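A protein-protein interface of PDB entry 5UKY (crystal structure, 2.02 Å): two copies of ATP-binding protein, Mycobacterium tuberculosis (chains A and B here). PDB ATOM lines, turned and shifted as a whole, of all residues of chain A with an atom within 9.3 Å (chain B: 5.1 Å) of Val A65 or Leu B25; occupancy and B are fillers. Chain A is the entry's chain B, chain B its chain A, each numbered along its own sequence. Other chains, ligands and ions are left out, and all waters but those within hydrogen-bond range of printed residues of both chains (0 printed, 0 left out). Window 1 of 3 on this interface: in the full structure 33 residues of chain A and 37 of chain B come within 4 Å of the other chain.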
ATOM      1  N   PHE A  17     -12.398  23.494  23.762  1.00  0.00           N
ATOM      2  CA  PHE A  17     -12.919  22.725  22.644  1.00  0.00           C
ATOM      3  C   PHE A  17     -14.077  21.818  23.026  1.00  0.00           C
ATOM      4  O   PHE A  17     -15.019  21.686  22.259  1.00  0.00           O
ATOM      5  CB  PHE A  17     -11.837  21.877  21.951  1.00  0.00           C
ATOM      6  CG  PHE A  17     -11.104  22.604  20.834  1.00  0.00           C
ATOM      7  CD1 PHE A  17     -11.776  22.987  19.673  1.00  0.00           C
ATOM      8  CD2 PHE A  17      -9.734  22.903  20.937  1.00  0.00           C
ATOM      9  CE1 PHE A  17     -11.102  23.654  18.651  1.00  0.00           C
ATOM     10  CE2 PHE A  17      -9.059  23.571  19.916  1.00  0.00           C
ATOM     11  CZ  PHE A  17      -9.744  23.947  18.771  1.00  0.00           C
ATOM     12  N   ILE A  18     -13.998  21.178  24.189  1.00  0.00           N
ATOM     13  CA  ILE A  18     -15.086  20.349  24.674  1.00  0.00           C
ATOM     14  C   ILE A  18     -16.300  21.212  24.735  1.00  0.00           C
ATOM     15  O   ILE A  18     -17.338  20.827  24.254  1.00  0.00           O
ATOM     16  CB  ILE A  18     -14.824  19.849  26.114  1.00  0.00           C
ATOM     17  CG1 ILE A  18     -13.760  18.793  26.103  1.00  0.00           C
ATOM     18  CG2 ILE A  18     -16.090  19.298  26.771  1.00  0.00           C
ATOM     19  CD1 ILE A  18     -13.218  18.503  27.487  1.00  0.00           C
ATOM     20  N   ALA A  21     -17.603  22.382  21.141  1.00  0.00           N
ATOM     21  CA  ALA A  21     -18.159  21.187  20.481  1.00  0.00           C
ATOM     22  C   ALA A  21     -19.488  20.776  21.109  1.00  0.00           C
ATOM     23  O   ALA A  21     -20.468  20.579  20.412  1.00  0.00           O
ATOM     24  CB  ALA A  21     -17.125  20.030  20.540  1.00  0.00           C
ATOM     25  N   SER A  22     -19.528  20.697  22.438  1.00  0.00           N
ATOM     26  CA  SER A  22     -20.724  20.329  23.132  1.00  0.00           C
ATOM     27  C   SER A  22     -21.870  21.315  22.840  1.00  0.00           C
ATOM     28  O   SER A  22     -23.002  20.886  22.597  1.00  0.00           O
ATOM     29  CB  SER A  22     -20.455  20.197  24.621  1.00  0.00           C
ATOM     30  OG  SER A  22     -19.550  19.135  24.831  1.00  0.00           O
ATOM     31  N   HIS A  23     -21.596  22.620  22.865  1.00  0.00           N
ATOM     32  CA  HIS A  23     -22.625  23.594  22.417  1.00  0.00           C
ATOM     33  C   HIS A  23     -23.079  23.399  20.994  1.00  0.00           C
ATOM     34  O   HIS A  23     -24.263  23.470  20.716  1.00  0.00           O
ATOM     35  CB  HIS A  23     -22.162  25.018  22.566  1.00  0.00           C
ATOM     36  CG  HIS A  23     -22.211  25.510  23.973  1.00  0.00           C
ATOM     37  ND1 HIS A  23     -21.090  25.912  24.647  1.00  0.00           N
ATOM     38  CD2 HIS A  23     -23.240  25.630  24.842  1.00  0.00           C
ATOM     39  CE1 HIS A  23     -21.424  26.291  25.865  1.00  0.00           C
ATOM     40  NE2 HIS A  23     -22.713  26.075  26.031  1.00  0.00           N
ATOM     41  N   GLU A  24     -22.137  23.144  20.101  1.00  0.00           N
ATOM     42  CA  GLU A  24     -22.413  22.906  18.664  1.00  0.00           C
ATOM     43  C   GLU A  24     -23.190  21.616  18.413  1.00  0.00           C
ATOM     44  O   GLU A  24     -23.734  21.461  17.348  1.00  0.00           O
ATOM     45  CB  GLU A  24     -21.103  22.708  17.906  1.00  0.00           C
ATOM     46  CG  GLU A  24     -20.940  23.502  16.657  1.00  0.00           C
ATOM     47  CD  GLU A  24     -20.515  24.894  16.995  1.00  0.00           C
ATOM     48  OE1 GLU A  24     -21.225  25.847  16.623  1.00  0.00           O
ATOM     49  OE2 GLU A  24     -19.470  25.026  17.650  1.00  0.00           O
ATOM     50  N   LEU A  25     -23.108  20.639  19.320  1.00  0.00           N
ATOM     51  CA  LEU A  25     -23.892  19.424  19.238  1.00  0.00           C
ATOM     52  C   LEU A  25     -25.294  19.640  19.801  1.00  0.00           C
ATOM     53  O   LEU A  25     -26.256  19.031  19.361  1.00  0.00           O
ATOM     54  CB  LEU A  25     -23.219  18.300  20.048  1.00  0.00           C
ATOM     55  CG  LEU A  25     -21.930  17.753  19.501  1.00  0.00           C
ATOM     56  CD1 LEU A  25     -21.314  16.830  20.530  1.00  0.00           C
ATOM     57  CD2 LEU A  25     -22.202  17.051  18.173  1.00  0.00           C
ATOM     58  N   ARG A  26     -25.402  20.481  20.805  1.00  0.00           N
ATOM     59  CA  ARG A  26     -26.684  20.743  21.423  1.00  0.00           C
ATOM     60  C   ARG A  26     -27.718  21.285  20.443  1.00  0.00           C
ATOM     61  O   ARG A  26     -28.893  20.874  20.437  1.00  0.00           O
ATOM     62  CB  ARG A  26     -26.470  21.630  22.676  1.00  0.00           C
ATOM     63  CG  ARG A  26     -27.643  21.686  23.613  1.00  0.00           C
ATOM     64  CD  ARG A  26     -27.255  21.508  25.063  1.00  0.00           C
ATOM     65  NE  ARG A  26     -26.703  22.695  25.703  1.00  0.00           N
ATOM     66  CZ  ARG A  26     -27.394  23.534  26.483  1.00  0.00           C
ATOM     67  NH1 ARG A  26     -28.701  23.366  26.679  1.00  0.00           N
ATOM     68  NH2 ARG A  26     -26.786  24.586  27.042  1.00  0.00           N
ATOM     69  N   LEU A  29     -29.226  18.640  17.953  1.00  0.00           N
ATOM     70  CA  LEU A  29     -30.086  17.814  18.795  1.00  0.00           C
ATOM     71  C   LEU A  29     -31.456  18.451  19.051  1.00  0.00           C
ATOM     72  O   LEU A  29     -32.533  17.777  18.994  1.00  0.00           O
ATOM     73  CB  LEU A  29     -29.374  17.492  20.108  1.00  0.00           C
ATOM     74  CG  LEU A  29     -28.210  16.483  19.994  1.00  0.00           C
ATOM     75  CD1 LEU A  29     -27.545  16.299  21.348  1.00  0.00           C
ATOM     76  CD2 LEU A  29     -28.608  15.120  19.397  1.00  0.00           C
ATOM     77  N   GLU A  57     -28.010  16.889   9.983  1.00  0.00           N
ATOM     78  CA  GLU A  57     -27.630  17.212  11.356  1.00  0.00           C
ATOM     79  C   GLU A  57     -26.725  16.109  11.974  1.00  0.00           C
ATOM     80  O   GLU A  57     -25.718  16.415  12.631  1.00  0.00           O
ATOM     81  CB  GLU A  57     -28.873  17.412  12.247  1.00  0.00           C
ATOM     82  CG  GLU A  57     -29.816  18.545  11.815  1.00  0.00           C
ATOM     83  CD  GLU A  57     -29.142  19.900  11.682  1.00  0.00           C
ATOM     84  OE1 GLU A  57     -28.224  20.205  12.466  1.00  0.00           O
ATOM     85  OE2 GLU A  57     -29.523  20.650  10.773  1.00  0.00           O
ATOM     86  N   ALA A  58     -27.083  14.848  11.733  1.00  0.00           N
ATOM     87  CA  ALA A  58     -26.315  13.720  12.273  1.00  0.00           C
ATOM     88  C   ALA A  58     -24.902  13.653  11.708  1.00  0.00           C
ATOM     89  O   ALA A  58     -23.954  13.387  12.444  1.00  0.00           O
ATOM     90  CB  ALA A  58     -27.055  12.434  12.013  1.00  0.00           C
ATOM     91  N   SER A  59     -24.759  13.928  10.409  1.00  0.00           N
ATOM     92  CA  SER A  59     -23.433  13.952   9.765  1.00  0.00           C
ATOM     93  C   SER A  59     -22.604  15.121  10.271  1.00  0.00           C
ATOM     94  O   SER A  59     -21.413  14.960  10.502  1.00  0.00           O
ATOM     95  CB  SER A  59     -23.532  13.978   8.249  1.00  0.00           C
ATOM     96  OG  SER A  59     -24.358  15.047   7.829  1.00  0.00           O
ATOM     97  N   ARG A  60     -23.236  16.258  10.537  1.00  0.00           N
ATOM     98  CA  ARG A  60     -22.510  17.383  11.159  1.00  0.00           C
ATOM     99  C   ARG A  60     -22.064  17.040  12.594  1.00  0.00           C
ATOM    100  O   ARG A  60     -20.933  17.333  13.016  1.00  0.00           O
ATOM    101  CB  ARG A  60     -23.367  18.644  11.162  1.00  0.00           C
ATOM    102  CG  ARG A  60     -22.575  19.930  11.084  1.00  0.00           C
ATOM    103  CD  ARG A  60     -23.375  20.993  10.340  1.00  0.00           C
ATOM    104  NE  ARG A  60     -24.683  21.190  10.953  1.00  0.00           N
ATOM    105  CZ  ARG A  60     -24.905  21.854  12.087  1.00  0.00           C
ATOM    106  NH1 ARG A  60     -23.900  22.435  12.752  1.00  0.00           N
ATOM    107  NH2 ARG A  60     -26.152  21.957  12.558  1.00  0.00           N
ATOM    108  N   MET A  61     -22.949  16.402  13.344  1.00  0.00           N
ATOM    109  CA  MET A  61     -22.559  15.952  14.677  1.00  0.00           C
ATOM    110  C   MET A  61     -21.390  14.952  14.587  1.00  0.00           C
ATOM    111  O   MET A  61     -20.403  15.072  15.335  1.00  0.00           O
ATOM    112  CB  MET A  61     -23.747  15.351  15.397  1.00  0.00           C
ATOM    113  CG  MET A  61     -24.826  16.367  15.741  1.00  0.00           C
ATOM    114  SD  MET A  61     -25.935  15.696  16.962  1.00  0.00           S
ATOM    115  CE  MET A  61     -26.864  14.570  15.963  1.00  0.00           C
ATOM    116  N   GLY A  62     -21.462  14.000  13.655  1.00  0.00           N
ATOM    117  CA  GLY A  62     -20.327  13.064  13.435  1.00  0.00           C
ATOM    118  C   GLY A  62     -19.004  13.743  13.173  1.00  0.00           C
ATOM    119  O   GLY A  62     -17.948  13.307  13.625  1.00  0.00           O
ATOM    120  N   LEU A  63     -19.038  14.841  12.431  1.00  0.00           N
ATOM    121  CA  LEU A  63     -17.797  15.605  12.203  1.00  0.00           C
ATOM    122  C   LEU A  63     -17.260  16.241  13.439  1.00  0.00           C
ATOM    123  O   LEU A  63     -16.057  16.230  13.677  1.00  0.00           O
ATOM    124  CB  LEU A  63     -17.989  16.697  11.129  1.00  0.00           C
ATOM    125  CG  LEU A  63     -18.157  16.097   9.720  1.00  0.00           C
ATOM    126  CD1 LEU A  63     -18.605  17.183   8.752  1.00  0.00           C
ATOM    127  CD2 LEU A  63     -16.876  15.425   9.241  1.00  0.00           C
ATOM    128  N   LEU A  64     -18.124  16.823  14.238  1.00  0.00           N
ATOM    129  CA  LEU A  64     -17.691  17.403  15.522  1.00  0.00           C
ATOM    130  C   LEU A  64     -17.101  16.351  16.490  1.00  0.00           C
ATOM    131  O   LEU A  64     -16.088  16.596  17.149  1.00  0.00           O
ATOM    132  CB  LEU A  64     -18.840  18.148  16.184  1.00  0.00           C
ATOM    133  CG  LEU A  64     -19.102  19.507  15.518  1.00  0.00           C
ATOM    134  CD1 LEU A  64     -20.566  19.907  15.697  1.00  0.00           C
ATOM    135  CD2 LEU A  64     -18.204  20.520  16.163  1.00  0.00           C
ATOM    136  N   VAL A  65     -17.739  15.198  16.564  1.00  0.00           N
ATOM    137  CA  VAL A  65     -17.298  14.105  17.451  1.00  0.00           C
ATOM    138  C   VAL A  65     -15.934  13.590  17.017  1.00  0.00           C
ATOM    139  O   VAL A  65     -15.068  13.406  17.849  1.00  0.00           O
ATOM    140  CB  VAL A  65     -18.371  12.977  17.528  1.00  0.00           C
ATOM    141  CG1 VAL A  65     -17.840  11.710  18.180  1.00  0.00           C
ATOM    142  CG2 VAL A  65     -19.609  13.486  18.286  1.00  0.00           C
ATOM    143  N   ASP A  66     -15.725  13.398  15.714  1.00  0.00           N
ATOM    144  CA  ASP A  66     -14.404  12.998  15.200  1.00  0.00           C
ATOM    145  C   ASP A  66     -13.325  14.068  15.388  1.00  0.00           C
ATOM    146  O   ASP A  66     -12.161  13.710  15.641  1.00  0.00           O
ATOM    147  CB  ASP A  66     -14.494  12.577  13.739  1.00  0.00           C
ATOM    148  CG  ASP A  66     -15.153  11.253  13.555  1.00  0.00           C
ATOM    149  OD1 ASP A  66     -15.486  10.576  14.529  1.00  0.00           O
ATOM    150  OD2 ASP A  66     -15.342  10.847  12.390  1.00  0.00           O
ATOM    151  N   ASP A  67     -13.687  15.362  15.331  1.00  0.00           N
ATOM    152  CA  ASP A  67     -12.744  16.414  15.708  1.00  0.00           C
ATOM    153  C   ASP A  67     -12.244  16.268  17.149  1.00  0.00           C
ATOM    154  O   ASP A  67     -11.072  16.479  17.441  1.00  0.00           O
ATOM    155  CB  ASP A  67     -13.333  17.814  15.596  1.00  0.00           C
ATOM    156  CG  ASP A  67     -13.653  18.228  14.159  1.00  0.00           C
ATOM    157  OD1 ASP A  67     -13.084  17.665  13.193  1.00  0.00           O
ATOM    158  OD2 ASP A  67     -14.483  19.152  14.002  1.00  0.00           O
ATOM    159  N   LEU A  68     -13.153  16.006  18.059  1.00  0.00           N
ATOM    160  CA  LEU A  68     -12.802  15.818  19.446  1.00  0.00           C
ATOM    161  C   LEU A  68     -11.824  14.643  19.553  1.00  0.00           C
ATOM    162  O   LEU A  68     -10.798  14.795  20.231  1.00  0.00           O
ATOM    163  CB  LEU A  68     -14.046  15.584  20.341  1.00  0.00           C
ATOM    164  CG  LEU A  68     -14.934  16.768  20.775  1.00  0.00           C
ATOM    165  CD1 LEU A  68     -16.234  16.358  21.470  1.00  0.00           C
ATOM    166  CD2 LEU A  68     -14.160  17.700  21.682  1.00  0.00           C
ATOM    167  N   LEU A  69     -12.128  13.520  18.876  1.00  0.00           N
ATOM    168  CA  LEU A  69     -11.312  12.295  18.930  1.00  0.00           C
ATOM    169  C   LEU A  69      -9.903  12.561  18.413  1.00  0.00           C
ATOM    170  O   LEU A  69      -8.923  12.139  19.018  1.00  0.00           O
ATOM    171  CB  LEU A  69     -11.957  11.120  18.162  1.00  0.00           C
ATOM    172  CG  LEU A  69     -13.217  10.463  18.755  1.00  0.00           C
ATOM    173  CD1 LEU A  69     -13.894   9.484  17.800  1.00  0.00           C
ATOM    174  CD2 LEU A  69     -12.873   9.738  20.071  1.00  0.00           C
ATOM    175  N   LEU A  70      -9.817  13.332  17.336  1.00  0.00           N
ATOM    176  CA  LEU A  70      -8.544  13.731  16.728  1.00  0.00           C
ATOM    177  C   LEU A  70      -7.757  14.719  17.600  1.00  0.00           C
ATOM    178  O   LEU A  70      -6.553  14.607  17.767  1.00  0.00           O
ATOM    179  CB  LEU A  70      -8.847  14.351  15.363  1.00  0.00           C
ATOM    180  CG  LEU A  70      -7.746  14.518  14.329  1.00  0.00           C
ATOM    181  CD1 LEU A  70      -6.954  13.225  14.184  1.00  0.00           C
ATOM    182  CD2 LEU A  70      -8.397  14.902  13.010  1.00  0.00           C
ATOM    183  N   LEU A  71      -8.440  15.713  18.141  1.00  0.00           N
ATOM    184  CA  LEU A  71      -7.815  16.619  19.086  1.00  0.00           C
ATOM    185  C   LEU A  71      -7.235  15.921  20.319  1.00  0.00           C
ATOM    186  O   LEU A  71      -6.169  16.320  20.800  1.00  0.00           O
ATOM    187  CB  LEU A  71      -8.818  17.663  19.525  1.00  0.00           C
ATOM    188  CG  LEU A  71      -8.319  18.726  20.488  1.00  0.00           C
ATOM    189  CD1 LEU A  71      -7.432  19.697  19.713  1.00  0.00           C
ATOM    190  CD2 LEU A  71      -9.495  19.428  21.153  1.00  0.00           C
ATOM    191  N   ALA A  72      -7.923  14.897  20.830  1.00  0.00           N
ATOM    192  CA  ALA A  72      -7.421  14.121  21.954  1.00  0.00           C
ATOM    193  C   ALA A  72      -6.132  13.384  21.578  1.00  0.00           C
ATOM    194  O   ALA A  72      -5.252  13.258  22.406  1.00  0.00           O
ATOM    195  CB  ALA A  72      -8.453  13.138  22.470  1.00  0.00           C
ATOM    196  N   ALA B  21     -15.434  10.258  26.329  1.00  0.00           N
ATOM    197  CA  ALA B  21     -16.638  11.082  26.133  1.00  0.00           C
ATOM    198  C   ALA B  21     -17.114  11.115  24.706  1.00  0.00           C
ATOM    199  O   ALA B  21     -18.288  11.010  24.455  1.00  0.00           O
ATOM    200  CB  ALA B  21     -16.403  12.482  26.641  1.00  0.00           C
ATOM    201  N   SER B  22     -16.201  11.252  23.762  1.00  0.00           N
ATOM    202  CA  SER B  22     -16.563  11.281  22.344  1.00  0.00           C
ATOM    203  C   SER B  22     -17.038   9.967  21.737  1.00  0.00           C
ATOM    204  O   SER B  22     -17.934   9.971  20.890  1.00  0.00           O
ATOM    205  CB  SER B  22     -15.352  11.745  21.544  1.00  0.00           C
ATOM    206  OG  SER B  22     -14.923  12.967  22.083  1.00  0.00           O
ATOM    207  N   HIS B  23     -16.416   8.851  22.134  1.00  0.00           N
ATOM    208  CA  HIS B  23     -16.882   7.531  21.709  1.00  0.00           C
ATOM    209  C   HIS B  23     -18.289   7.257  22.250  1.00  0.00           C
ATOM    210  O   HIS B  23     -19.096   6.618  21.562  1.00  0.00           O
ATOM    211  CB  HIS B  23     -15.914   6.423  22.168  1.00  0.00           C
ATOM    212  CG  HIS B  23     -14.676   6.289  21.316  1.00  0.00           C
ATOM    213  ND1 HIS B  23     -13.403   6.389  21.830  1.00  0.00           N
ATOM    214  CD2 HIS B  23     -14.525   5.995  20.003  1.00  0.00           C
ATOM    215  CE1 HIS B  23     -12.521   6.195  20.863  1.00  0.00           C
ATOM    216  NE2 HIS B  23     -13.178   5.967  19.743  1.00  0.00           N
ATOM    217  N   GLU B  24     -18.573   7.726  23.462  1.00  0.00           N
ATOM    218  CA  GLU B  24     -19.910   7.589  24.062  1.00  0.00           C
ATOM    219  C   GLU B  24     -20.998   8.349  23.221  1.00  0.00           C
ATOM    220  O   GLU B  24     -22.089   7.889  23.052  1.00  0.00           O
ATOM    221  CB  GLU B  24     -19.904   8.142  25.477  1.00  0.00           C
ATOM    222  CG  GLU B  24     -19.286   7.215  26.537  1.00  0.00           C
ATOM    223  CD  GLU B  24     -19.164   7.862  27.890  1.00  0.00           C
ATOM    224  OE1 GLU B  24     -19.642   9.011  28.094  1.00  0.00           O
ATOM    225  OE2 GLU B  24     -18.551   7.239  28.761  1.00  0.00           O
ATOM    226  N   LEU B  25     -20.629   9.503  22.704  1.00  0.00           N
ATOM    227  CA  LEU B  25     -21.450  10.265  21.763  1.00  0.00           C
ATOM    228  C   LEU B  25     -21.609   9.553  20.435  1.00  0.00           C
ATOM    229  O   LEU B  25     -22.705   9.578  19.855  1.00  0.00           O
ATOM    230  CB  LEU B  25     -20.855  11.661  21.542  1.00  0.00           C
ATOM    231  CG  LEU B  25     -20.879  12.554  22.783  1.00  0.00           C
ATOM    232  CD1 LEU B  25     -19.825  13.655  22.600  1.00  0.00           C
ATOM    233  CD2 LEU B  25     -22.278  13.118  22.964  1.00  0.00           C
ATOM    234  N   ARG B  26     -20.542   8.908  19.983  1.00  0.00           N
ATOM    235  CA  ARG B  26     -20.538   8.141  18.697  1.00  0.00           C
ATOM    236  C   ARG B  26     -21.678   7.095  18.564  1.00  0.00           C
ATOM    237  O   ARG B  26     -22.341   7.004  17.527  1.00  0.00           O
ATOM    238  CB  ARG B  26     -19.187   7.470  18.458  1.00  0.00           C
ATOM    239  CG  ARG B  26     -18.475   7.916  17.203  1.00  0.00           C
ATOM    240  CD  ARG B  26     -17.357   6.983  16.798  1.00  0.00           C
ATOM    241  NE  ARG B  26     -16.536   7.679  15.815  1.00  0.00           N
ATOM    242  CZ  ARG B  26     -15.300   7.338  15.427  1.00  0.00           C
ATOM    243  NH1 ARG B  26     -14.674   8.093  14.523  1.00  0.00           N
ATOM    244  NH2 ARG B  26     -14.672   6.268  15.923  1.00  0.00           N
ATOM    245  N   THR B  27     -21.958   6.381  19.640  1.00  0.00           N
ATOM    246  CA  THR B  27     -22.896   5.274  19.603  1.00  0.00           C
ATOM    247  C   THR B  27     -24.395   5.651  19.377  1.00  0.00           C
ATOM    248  O   THR B  27     -25.028   5.102  18.504  1.00  0.00           O
ATOM    249  CB  THR B  27     -22.675   4.407  20.848  1.00  0.00           C
ATOM    250  OG1 THR B  27     -21.279   4.091  20.901  1.00  0.00           O
ATOM    251  CG2 THR B  27     -23.488   3.127  20.775  1.00  0.00           C
ATOM    252  N   PRO B  28     -24.968   6.571  20.170  1.00  0.00           N
ATOM    253  CA  PRO B  28     -26.274   7.103  19.721  1.00  0.00           C
ATOM    254  C   PRO B  28     -26.277   7.711  18.304  1.00  0.00           C
ATOM    255  O   PRO B  28     -27.235   7.496  17.567  1.00  0.00           O
ATOM    256  CB  PRO B  28     -26.616   8.154  20.759  1.00  0.00           C
ATOM    257  CG  PRO B  28     -25.391   8.349  21.581  1.00  0.00           C
ATOM    258  CD  PRO B  28     -24.571   7.102  21.471  1.00  0.00           C
ATOM    259  N   LEU B  29     -25.252   8.478  17.930  1.00  0.00           N
ATOM    260  CA  LEU B  29     -25.190   9.051  16.597  1.00  0.00           C
ATOM    261  C   LEU B  29     -25.235   8.059  15.450  1.00  0.00           C
ATOM    262  O   LEU B  29     -25.781   8.368  14.379  1.00  0.00           O
ATOM    263  CB  LEU B  29     -23.879   9.804  16.369  1.00  0.00           C
ATOM    264  CG  LEU B  29     -23.893  11.273  16.306  1.00  0.00           C
ATOM    265  CD1 LEU B  29     -22.473  11.858  16.194  1.00  0.00           C
ATOM    266  CD2 LEU B  29     -24.838  11.660  15.170  1.00  0.00           C
ATOM    267  N   MET B  61     -28.256  11.442  23.897  1.00  0.00           N
ATOM    268  CA  MET B  61     -27.152  12.234  23.486  1.00  0.00           C
ATOM    269  C   MET B  61     -27.182  13.632  24.135  1.00  0.00           C
ATOM    270  O   MET B  61     -26.194  14.171  24.509  1.00  0.00           O
ATOM    271  CB  MET B  61     -27.205  12.329  21.992  1.00  0.00           C
ATOM    272  CG  MET B  61     -25.873  12.401  21.354  1.00  0.00           C
ATOM    273  SD  MET B  61     -25.854  12.201  19.602  1.00  0.00           S
ATOM    274  CE  MET B  61     -24.395  13.166  19.329  1.00  0.00           C
ATOM    275  N   LEU B  64     -25.901  13.322  27.638  1.00  0.00           N
ATOM    276  CA  LEU B  64     -24.422  13.197  27.591  1.00  0.00           C
ATOM    277  C   LEU B  64     -23.736  14.549  27.358  1.00  0.00           C
ATOM    278  O   LEU B  64     -22.736  14.850  27.977  1.00  0.00           O
ATOM    279  CB  LEU B  64     -24.007  12.235  26.502  1.00  0.00           C
ATOM    280  CG  LEU B  64     -24.300  10.748  26.712  1.00  0.00           C
ATOM    281  CD1 LEU B  64     -23.928  10.038  25.425  1.00  0.00           C
ATOM    282  CD2 LEU B  64     -23.527  10.113  27.888  1.00  0.00           C
ATOM    283  N   VAL B  65     -24.294  15.350  26.443  1.00  0.00           N
ATOM    284  CA  VAL B  65     -23.774  16.676  26.083  1.00  0.00           C
ATOM    285  C   VAL B  65     -23.965  17.658  27.253  1.00  0.00           C
ATOM    286  O   VAL B  65     -23.055  18.324  27.610  1.00  0.00           O
ATOM    287  CB  VAL B  65     -24.407  17.209  24.742  1.00  0.00           C
ATOM    288  CG1 VAL B  65     -24.092  18.677  24.516  1.00  0.00           C
ATOM    289  CG2 VAL B  65     -23.942  16.413  23.556  1.00  0.00           C
ATOM    290  N   LEU B  68     -21.275  16.791  29.708  1.00  0.00           N
ATOM    291  CA  LEU B  68     -20.008  17.316  29.236  1.00  0.00           C
ATOM    292  C   LEU B  68     -19.817  18.798  29.463  1.00  0.00           C
ATOM    293  O   LEU B  68     -18.732  19.240  29.893  1.00  0.00           O
ATOM    294  CB  LEU B  68     -19.783  17.047  27.743  1.00  0.00           C
ATOM    295  CG  LEU B  68     -19.341  15.638  27.425  1.00  0.00           C
ATOM    296  CD1 LEU B  68     -19.347  15.384  25.922  1.00  0.00           C
ATOM    297  CD2 LEU B  68     -17.971  15.357  28.073  1.00  0.00           C
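O of Ser A22 touches CG1 of Val B65 (3.1 Å).
Leu B68 touches Ser A22 (CB to OG, 3.6 Å).
O of Ala A58 touches CD2 of Leu B29, at 3.3 Å.
Met A61 touches Leu B29.
Met A61 touches Met B61.
Leu B29 touches Gly A62.
CG1 of Val A65 touches CG of Arg B26, 3.97 Å away.
Ser B22 touches Leu A68 (OG to CB, 3.3 Å).
Ser B22 touches Leu A69.
CD1 of Leu A69 touches CZ of Arg B26, at 3.5 Å.
NH1 of Arg B26 is in salt-bridge range of OD1 of Asp A66.
Of the printed residues of chain B, Leu A29 touches Met B61.
Of the printed residues of chain B, Met A61 touches Leu B29 (3.6 Å) and Met B61 (3.8 Å).
Of the printed residues of chain B, Leu A68 touches Ser B22.
Ser B22 touches just these residues of chain A: Val A65, Leu A68 and Leu A69.
Of the printed residues of chain A, His B23 touches Leu A69.
Of the printed residues of chain A, Met B61 touches Leu A29 (3.9 Å) and Met A61 (3.8 Å).
The nearest residue of chain B that does not touch Val A65 is Met B61 (4.9 Å).
The nearest residue of chain A that does not touch Leu B25 is Leu A25 (4.1 Å).
The nearest printed residue of chain A that does not touch Val B65 is Leu A25 (4.03 Å).
O of His B23 is in hydrogen-bond range of OG1 of Thr B27 (3.4 Å).
The side-chain hydroxyl of Ser A22 sits at hydrogen-bond distance from the backbone carbonyl oxygen of Ile A18 (2.8 Å).
Hydrophobic or aromatic side chains of chain A that line the printed part of chain B: Leu A29, Ala A58, Met A61, Val A65, Leu A68 and Leu A69.
Along chain B the printed residues that touch a printed residue of chain A span positions 22 to 68.
Among the printed residues, Asp or Glu carboxylates within 4 Å of a Lys or Arg side-chain nitrogen of the other chain: Asp A66 with Arg B26.
Ser A22 touches Val B65, and with the chains exchanged Val A65 touches Ser B22.
Met A61 touches its own counterpart, Met B61.
Val A65 touches Arg B26, but with the chains exchanged Arg A26 does not touch Val B65 (4.2 Å).
Val A65 touches Leu B29, but with the chains exchanged Leu A29 does not touch Val B65 (4.2 Å).
Of the 16 pairs that touch across the chains among the printed residues, 7 have their exchanged pair printed and touching as well.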
